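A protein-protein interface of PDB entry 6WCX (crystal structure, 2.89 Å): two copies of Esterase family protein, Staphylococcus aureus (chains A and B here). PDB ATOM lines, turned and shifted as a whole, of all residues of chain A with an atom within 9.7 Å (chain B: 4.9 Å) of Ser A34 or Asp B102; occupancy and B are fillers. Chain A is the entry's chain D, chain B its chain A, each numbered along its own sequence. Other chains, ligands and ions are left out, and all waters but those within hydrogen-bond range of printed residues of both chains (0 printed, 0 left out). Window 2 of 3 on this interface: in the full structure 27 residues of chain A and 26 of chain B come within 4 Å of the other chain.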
ATOM      1  N   ASP A  28       2.503   7.236  33.990  1.00  0.00           N
ATOM      2  CA  ASP A  28       2.863   5.833  34.096  1.00  0.00           C
ATOM      3  C   ASP A  28       3.743   5.444  32.917  1.00  0.00           C
ATOM      4  O   ASP A  28       3.678   6.054  31.847  1.00  0.00           O
ATOM      5  CB  ASP A  28       1.623   4.941  34.108  1.00  0.00           C
ATOM      6  CG  ASP A  28       1.931   3.529  34.546  1.00  0.00           C
ATOM      7  OD1 ASP A  28       1.807   3.243  35.757  1.00  0.00           O
ATOM      8  OD2 ASP A  28       2.343   2.722  33.683  1.00  0.00           O
ATOM      9  N   GLN A  29       4.555   4.396  33.117  1.00  0.00           N
ATOM     10  CA  GLN A  29       5.500   3.971  32.085  1.00  0.00           C
ATOM     11  C   GLN A  29       4.793   3.315  30.901  1.00  0.00           C
ATOM     12  O   GLN A  29       5.296   3.388  29.772  1.00  0.00           O
ATOM     13  CB  GLN A  29       6.541   3.027  32.690  1.00  0.00           C
ATOM     14  CG  GLN A  29       7.831   2.920  31.882  1.00  0.00           C
ATOM     15  CD  GLN A  29       8.509   1.546  32.011  1.00  0.00           C
ATOM     16  OE1 GLN A  29       7.824   0.518  32.084  1.00  0.00           O
ATOM     17  NE2 GLN A  29       9.853   1.527  32.032  1.00  0.00           N
ATOM     18  N   SER A  30       3.638   2.670  31.142  1.00  0.00           N
ATOM     19  CA  SER A  30       2.756   2.189  30.072  1.00  0.00           C
ATOM     20  C   SER A  30       2.431   3.264  29.041  1.00  0.00           C
ATOM     21  O   SER A  30       2.304   2.961  27.849  1.00  0.00           O
ATOM     22  CB  SER A  30       1.469   1.596  30.652  1.00  0.00           C
ATOM     23  OG  SER A  30       0.821   2.481  31.543  1.00  0.00           O
ATOM     24  N   PHE A  31       2.266   4.520  29.487  1.00  0.00           N
ATOM     25  CA  PHE A  31       1.770   5.596  28.628  1.00  0.00           C
ATOM     26  C   PHE A  31       2.758   5.976  27.537  1.00  0.00           C
ATOM     27  O   PHE A  31       2.344   6.511  26.507  1.00  0.00           O
ATOM     28  CB  PHE A  31       1.462   6.855  29.441  1.00  0.00           C
ATOM     29  CG  PHE A  31       0.391   6.677  30.489  1.00  0.00           C
ATOM     30  CD1 PHE A  31      -0.533   5.645  30.413  1.00  0.00           C
ATOM     31  CD2 PHE A  31       0.317   7.562  31.557  1.00  0.00           C
ATOM     32  CE1 PHE A  31      -1.481   5.493  31.383  1.00  0.00           C
ATOM     33  CE2 PHE A  31      -0.640   7.416  32.529  1.00  0.00           C
ATOM     34  CZ  PHE A  31      -1.543   6.383  32.440  1.00  0.00           C
ATOM     35  N   PHE A  32       4.047   5.725  27.749  1.00  0.00           N
ATOM     36  CA  PHE A  32       5.090   6.119  26.813  1.00  0.00           C
ATOM     37  C   PHE A  32       5.566   4.962  25.945  1.00  0.00           C
ATOM     38  O   PHE A  32       6.350   5.185  25.016  1.00  0.00           O
ATOM     39  CB  PHE A  32       6.279   6.716  27.578  1.00  0.00           C
ATOM     40  CG  PHE A  32       5.982   8.052  28.201  1.00  0.00           C
ATOM     41  CD1 PHE A  32       5.866   9.189  27.410  1.00  0.00           C
ATOM     42  CD2 PHE A  32       5.792   8.168  29.573  1.00  0.00           C
ATOM     43  CE1 PHE A  32       5.578  10.416  27.979  1.00  0.00           C
ATOM     44  CE2 PHE A  32       5.498   9.392  30.148  1.00  0.00           C
ATOM     45  CZ  PHE A  32       5.387  10.517  29.350  1.00  0.00           C
ATOM     46  N   ASN A  33       5.075   3.748  26.190  1.00  0.00           N
ATOM     47  CA  ASN A  33       5.482   2.561  25.450  1.00  0.00           C
ATOM     48  C   ASN A  33       4.317   2.042  24.623  1.00  0.00           C
ATOM     49  O   ASN A  33       3.276   1.652  25.170  1.00  0.00           O
ATOM     50  CB  ASN A  33       5.990   1.475  26.393  1.00  0.00           C
ATOM     51  CG  ASN A  33       6.961   0.530  25.715  1.00  0.00           C
ATOM     52  OD1 ASN A  33       6.746   0.094  24.583  1.00  0.00           O
ATOM     53  ND2 ASN A  33       8.058   0.237  26.398  1.00  0.00           N
ATOM     54  N   SER A  34       4.517   2.005  23.308  1.00  0.00           N
ATOM     55  CA  SER A  34       3.472   1.612  22.376  1.00  0.00           C
ATOM     56  C   SER A  34       3.173   0.120  22.407  1.00  0.00           C
ATOM     57  O   SER A  34       2.065  -0.277  22.035  1.00  0.00           O
ATOM     58  CB  SER A  34       3.890   2.005  20.951  1.00  0.00           C
ATOM     59  OG  SER A  34       5.194   1.493  20.631  1.00  0.00           O
ATOM     60  N   ASP A  35       4.113  -0.700  22.882  1.00  0.00           N
ATOM     61  CA  ASP A  35       3.994  -2.154  22.855  1.00  0.00           C
ATOM     62  C   ASP A  35       3.374  -2.755  24.115  1.00  0.00           C
ATOM     63  O   ASP A  35       3.100  -3.963  24.130  1.00  0.00           O
ATOM     64  CB  ASP A  35       5.379  -2.766  22.609  1.00  0.00           C
ATOM     65  CG  ASP A  35       5.822  -2.628  21.164  1.00  0.00           C
ATOM     66  OD1 ASP A  35       4.945  -2.428  20.288  1.00  0.00           O
ATOM     67  OD2 ASP A  35       7.052  -2.643  20.917  1.00  0.00           O
ATOM     68  N   THR A  36       3.168  -1.962  25.168  1.00  0.00           N
ATOM     69  CA  THR A  36       2.589  -2.445  26.414  1.00  0.00           C
ATOM     70  C   THR A  36       1.129  -2.022  26.509  1.00  0.00           C
ATOM     71  O   THR A  36       0.700  -1.041  25.891  1.00  0.00           O
ATOM     72  CB  THR A  36       3.364  -1.941  27.641  1.00  0.00           C
ATOM     73  OG1 THR A  36       3.284  -0.513  27.720  1.00  0.00           O
ATOM     74  CG2 THR A  36       4.819  -2.358  27.562  1.00  0.00           C
ATOM     75  N   THR A  37       0.356  -2.788  27.267  1.00  0.00           N
ATOM     76  CA  THR A  37      -1.003  -2.364  27.564  1.00  0.00           C
ATOM     77  C   THR A  37      -0.971  -1.269  28.623  1.00  0.00           C
ATOM     78  O   THR A  37      -0.045  -1.192  29.438  1.00  0.00           O
ATOM     79  CB  THR A  37      -1.877  -3.538  28.030  1.00  0.00           C
ATOM     80  OG1 THR A  37      -1.698  -3.758  29.436  1.00  0.00           O
ATOM     81  CG2 THR A  37      -1.524  -4.819  27.264  1.00  0.00           C
ATOM     82  N   VAL A  38      -1.955  -0.379  28.562  1.00  0.00           N
ATOM     83  CA  VAL A  38      -2.017   0.729  29.506  1.00  0.00           C
ATOM     84  C   VAL A  38      -2.491   0.203  30.864  1.00  0.00           C
ATOM     85  O   VAL A  38      -3.379  -0.657  30.954  1.00  0.00           O
ATOM     86  CB  VAL A  38      -2.906   1.870  28.946  1.00  0.00           C
ATOM     87  CG1 VAL A  38      -2.492   2.212  27.512  1.00  0.00           C
ATOM     88  CG2 VAL A  38      -4.409   1.547  28.948  1.00  0.00           C
ATOM     89  N   LEU B  98       7.879  11.334  18.151  1.00  0.00           N
ATOM     90  CA  LEU B  98       7.525   9.932  18.354  1.00  0.00           C
ATOM     91  C   LEU B  98       7.034   9.688  19.773  1.00  0.00           C
ATOM     92  O   LEU B  98       6.159   8.845  19.986  1.00  0.00           O
ATOM     93  CB  LEU B  98       8.721   9.027  18.054  1.00  0.00           C
ATOM     94  CG  LEU B  98       9.416   9.200  16.701  1.00  0.00           C
ATOM     95  CD1 LEU B  98      10.666   8.349  16.627  1.00  0.00           C
ATOM     96  CD2 LEU B  98       8.465   8.877  15.549  1.00  0.00           C
ATOM     97  N   GLU B  99       7.560  10.434  20.746  1.00  0.00           N
ATOM     98  CA  GLU B  99       7.070  10.310  22.112  1.00  0.00           C
ATOM     99  C   GLU B  99       5.672  10.891  22.252  1.00  0.00           C
ATOM    100  O   GLU B  99       4.826  10.289  22.922  1.00  0.00           O
ATOM    101  CB  GLU B  99       8.022  10.983  23.098  1.00  0.00           C
ATOM    102  CG  GLU B  99       7.582  10.792  24.534  1.00  0.00           C
ATOM    103  CD  GLU B  99       7.931  11.958  25.418  1.00  0.00           C
ATOM    104  OE1 GLU B  99       7.122  12.913  25.510  1.00  0.00           O
ATOM    105  OE2 GLU B  99       9.017  11.897  26.032  1.00  0.00           O
ATOM    106  N   VAL B 100       5.425  12.074  21.659  1.00  0.00           N
ATOM    107  CA  VAL B 100       4.076  12.655  21.649  1.00  0.00           C
ATOM    108  C   VAL B 100       3.086  11.706  20.983  1.00  0.00           C
ATOM    109  O   VAL B 100       1.991  11.468  21.514  1.00  0.00           O
ATOM    110  CB  VAL B 100       4.069  14.041  20.968  1.00  0.00           C
ATOM    111  CG1 VAL B 100       2.647  14.589  20.874  1.00  0.00           C
ATOM    112  CG2 VAL B 100       4.899  15.015  21.749  1.00  0.00           C
ATOM    113  N   TYR B 101       3.485  11.115  19.842  1.00  0.00           N
ATOM    114  CA  TYR B 101       2.663  10.129  19.137  1.00  0.00           C
ATOM    115  C   TYR B 101       2.334   8.943  20.032  1.00  0.00           C
ATOM    116  O   TYR B 101       1.165   8.557  20.157  1.00  0.00           O
ATOM    117  CB  TYR B 101       3.387   9.653  17.873  1.00  0.00           C
ATOM    118  CG  TYR B 101       2.579   8.747  16.958  1.00  0.00           C
ATOM    119  CD1 TYR B 101       2.537   7.364  17.164  1.00  0.00           C
ATOM    120  CD2 TYR B 101       1.903   9.263  15.860  1.00  0.00           C
ATOM    121  CE1 TYR B 101       1.813   6.534  16.343  1.00  0.00           C
ATOM    122  CE2 TYR B 101       1.177   8.426  15.015  1.00  0.00           C
ATOM    123  CZ  TYR B 101       1.140   7.062  15.273  1.00  0.00           C
ATOM    124  OH  TYR B 101       0.439   6.209  14.454  1.00  0.00           O
ATOM    125  N   ASP B 102       3.357   8.370  20.680  1.00  0.00           N
ATOM    126  CA  ASP B 102       3.142   7.226  21.562  1.00  0.00           C
ATOM    127  C   ASP B 102       2.289   7.601  22.767  1.00  0.00           C
ATOM    128  O   ASP B 102       1.431   6.818  23.184  1.00  0.00           O
ATOM    129  CB  ASP B 102       4.477   6.656  22.035  1.00  0.00           C
ATOM    130  CG  ASP B 102       5.151   5.805  20.986  1.00  0.00           C
ATOM    131  OD1 ASP B 102       4.630   5.747  19.847  1.00  0.00           O
ATOM    132  OD2 ASP B 102       6.193   5.185  21.307  1.00  0.00           O
ATOM    133  N   TYR B 103       2.479   8.811  23.301  1.00  0.00           N
ATOM    134  CA  TYR B 103       1.779   9.227  24.514  1.00  0.00           C
ATOM    135  C   TYR B 103       0.278   9.391  24.275  1.00  0.00           C
ATOM    136  O   TYR B 103      -0.539   8.901  25.061  1.00  0.00           O
ATOM    137  CB  TYR B 103       2.382  10.529  25.022  1.00  0.00           C
ATOM    138  CG  TYR B 103       1.800  11.040  26.306  1.00  0.00           C
ATOM    139  CD1 TYR B 103       2.104  10.443  27.519  1.00  0.00           C
ATOM    140  CD2 TYR B 103       0.943  12.127  26.305  1.00  0.00           C
ATOM    141  CE1 TYR B 103       1.569  10.930  28.705  1.00  0.00           C
ATOM    142  CE2 TYR B 103       0.406  12.610  27.469  1.00  0.00           C
ATOM    143  CZ  TYR B 103       0.717  12.018  28.664  1.00  0.00           C
ATOM    144  OH  TYR B 103       0.166  12.524  29.819  1.00  0.00           O
ATOM    145  N   VAL B 104      -0.104  10.088  23.201  1.00  0.00           N
ATOM    146  CA  VAL B 104      -1.526  10.339  22.968  1.00  0.00           C
ATOM    147  C   VAL B 104      -2.255   9.119  22.412  1.00  0.00           C
ATOM    148  O   VAL B 104      -3.483   9.044  22.523  1.00  0.00           O
ATOM    149  CB  VAL B 104      -1.739  11.563  22.063  1.00  0.00           C
ATOM    150  CG1 VAL B 104      -1.152  12.796  22.727  1.00  0.00           C
ATOM    151  CG2 VAL B 104      -1.155  11.344  20.671  1.00  0.00           C
ATOM    152  N   HIS B 105      -1.552   8.165  21.799  1.00  0.00           N
ATOM    153  CA  HIS B 105      -2.249   6.954  21.388  1.00  0.00           C
ATOM    154  C   HIS B 105      -2.519   6.043  22.580  1.00  0.00           C
ATOM    155  O   HIS B 105      -3.513   5.305  22.579  1.00  0.00           O
ATOM    156  CB  HIS B 105      -1.458   6.235  20.297  1.00  0.00           C
ATOM    157  CG  HIS B 105      -1.665   6.815  18.931  1.00  0.00           C
ATOM    158  ND1 HIS B 105      -1.031   7.964  18.504  1.00  0.00           N
ATOM    159  CD2 HIS B 105      -2.446   6.413  17.899  1.00  0.00           C
ATOM    160  CE1 HIS B 105      -1.409   8.243  17.267  1.00  0.00           C
ATOM    161  NE2 HIS B 105      -2.270   7.319  16.877  1.00  0.00           N
ATOM    162  N   GLN B 106      -1.692   6.130  23.629  1.00  0.00           N
ATOM    163  CA  GLN B 106      -1.913   5.324  24.825  1.00  0.00           C
ATOM    164  C   GLN B 106      -2.988   5.922  25.737  1.00  0.00           C
ATOM    165  O   GLN B 106      -3.767   5.177  26.342  1.00  0.00           O
ATOM    166  CB  GLN B 106      -0.608   5.156  25.604  1.00  0.00           C
ATOM    167  CG  GLN B 106       0.458   4.321  24.929  1.00  0.00           C
ATOM    168  CD  GLN B 106       0.130   2.852  24.877  1.00  0.00           C
ATOM    169  OE1 GLN B 106      -0.407   2.361  23.881  1.00  0.00           O
ATOM    170  NE2 GLN B 106       0.470   2.128  25.943  1.00  0.00           N
ATOM    171  N   LYS B 139       4.052   4.628  10.317  1.00  0.00           N
ATOM    172  CA  LYS B 139       3.142   5.251  11.272  1.00  0.00           C
ATOM    173  C   LYS B 139       2.082   6.119  10.617  1.00  0.00           C
ATOM    174  O   LYS B 139       1.122   6.499  11.295  1.00  0.00           O
ATOM    175  CB  LYS B 139       3.904   6.113  12.287  1.00  0.00           C
ATOM    176  CG  LYS B 139       4.529   5.353  13.446  1.00  0.00           C
ATOM    177  CD  LYS B 139       5.140   6.320  14.464  1.00  0.00           C
ATOM    178  CE  LYS B 139       5.969   5.580  15.505  1.00  0.00           C
ATOM    179  NZ  LYS B 139       7.111   4.881  14.853  1.00  0.00           N
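The side-chain carboxylate (OD2) of Asp A28 lies within hydrogen-bond range of the side-chain hydroxyl (OG) of Ser A30 (2.6 Å). OD1 of Asn A33 is in hydrogen-bond range of N of Asp A35, at 3.2 Å. O of Asn A33 sits at hydrogen-bond distance from OG1 of Thr A36, 3.3 Å away.
Of the printed residues of chain B, Ser A30 touches Gln B106. Of chain B, only Asp B102 (3.9 Å) comes within 4 Å of Ser A34. Printed residues of chain B within 4 Å of Thr A36: Gln B106. Thr A37 touches none of the printed residues of chain B. Leu B98 touches none of the printed residues of chain A. Of the printed residues of chain A, Asp B102 touches Phe A31 (3.5 Å), Phe A32 (3.7 Å) and Ser A34 (3.9 Å). The nearest residue of chain A that does not touch Asp B102 is Asn A33 (4.9 Å).
No position is printed for both chains. Of the 11 pairs that touch across the chains among the printed residues, none has its exchanged pair printed and touching as well.
Printed residues of chain B that touch a printed residue of chain A: Glu B99, Asp B102, Tyr B103 and Gln B106. Along chain B the printed residues that touch a printed residue of chain A span positions 99 to 106. Hydrophobic or aromatic side chains of chain A that line the printed part of chain B: Phe A32 and Val A38. Among the printed residues, no Asp or Glu carboxylate lies within 4 Å of a Lys or Arg side-chain nitrogen of the other chain.
Phe A31 touches Tyr B103 (O to CA, 3.4 Å). Gln B106 touches Phe A31 (CG to O, 3.3 Å). Glu B99 touches Phe A32. O of Phe A32 touches OD2 of Asp B102, 3.7 Å away. CE1 of Phe A32 touches CD1 of Tyr B103 (3.5 Å). Asp B102 touches Ser A34 (OD2 to OG, 3.9 Å). Val A38 touches Gln B106.
NE2 of Gln B106 is in hydrogen-bond range of O of Ser A30 (2.8 Å). NE2 of Gln B106 is in hydrogen-bond range of O of Asn A33, at 2.9 Å. The side-chain amide nitrogen of Gln B106 is in hydrogen-bond range of the backbone carbonyl oxygen of Thr A36 (3.2 Å). O of Phe A31 sits close to O of Asp B102 (3.5 Å).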
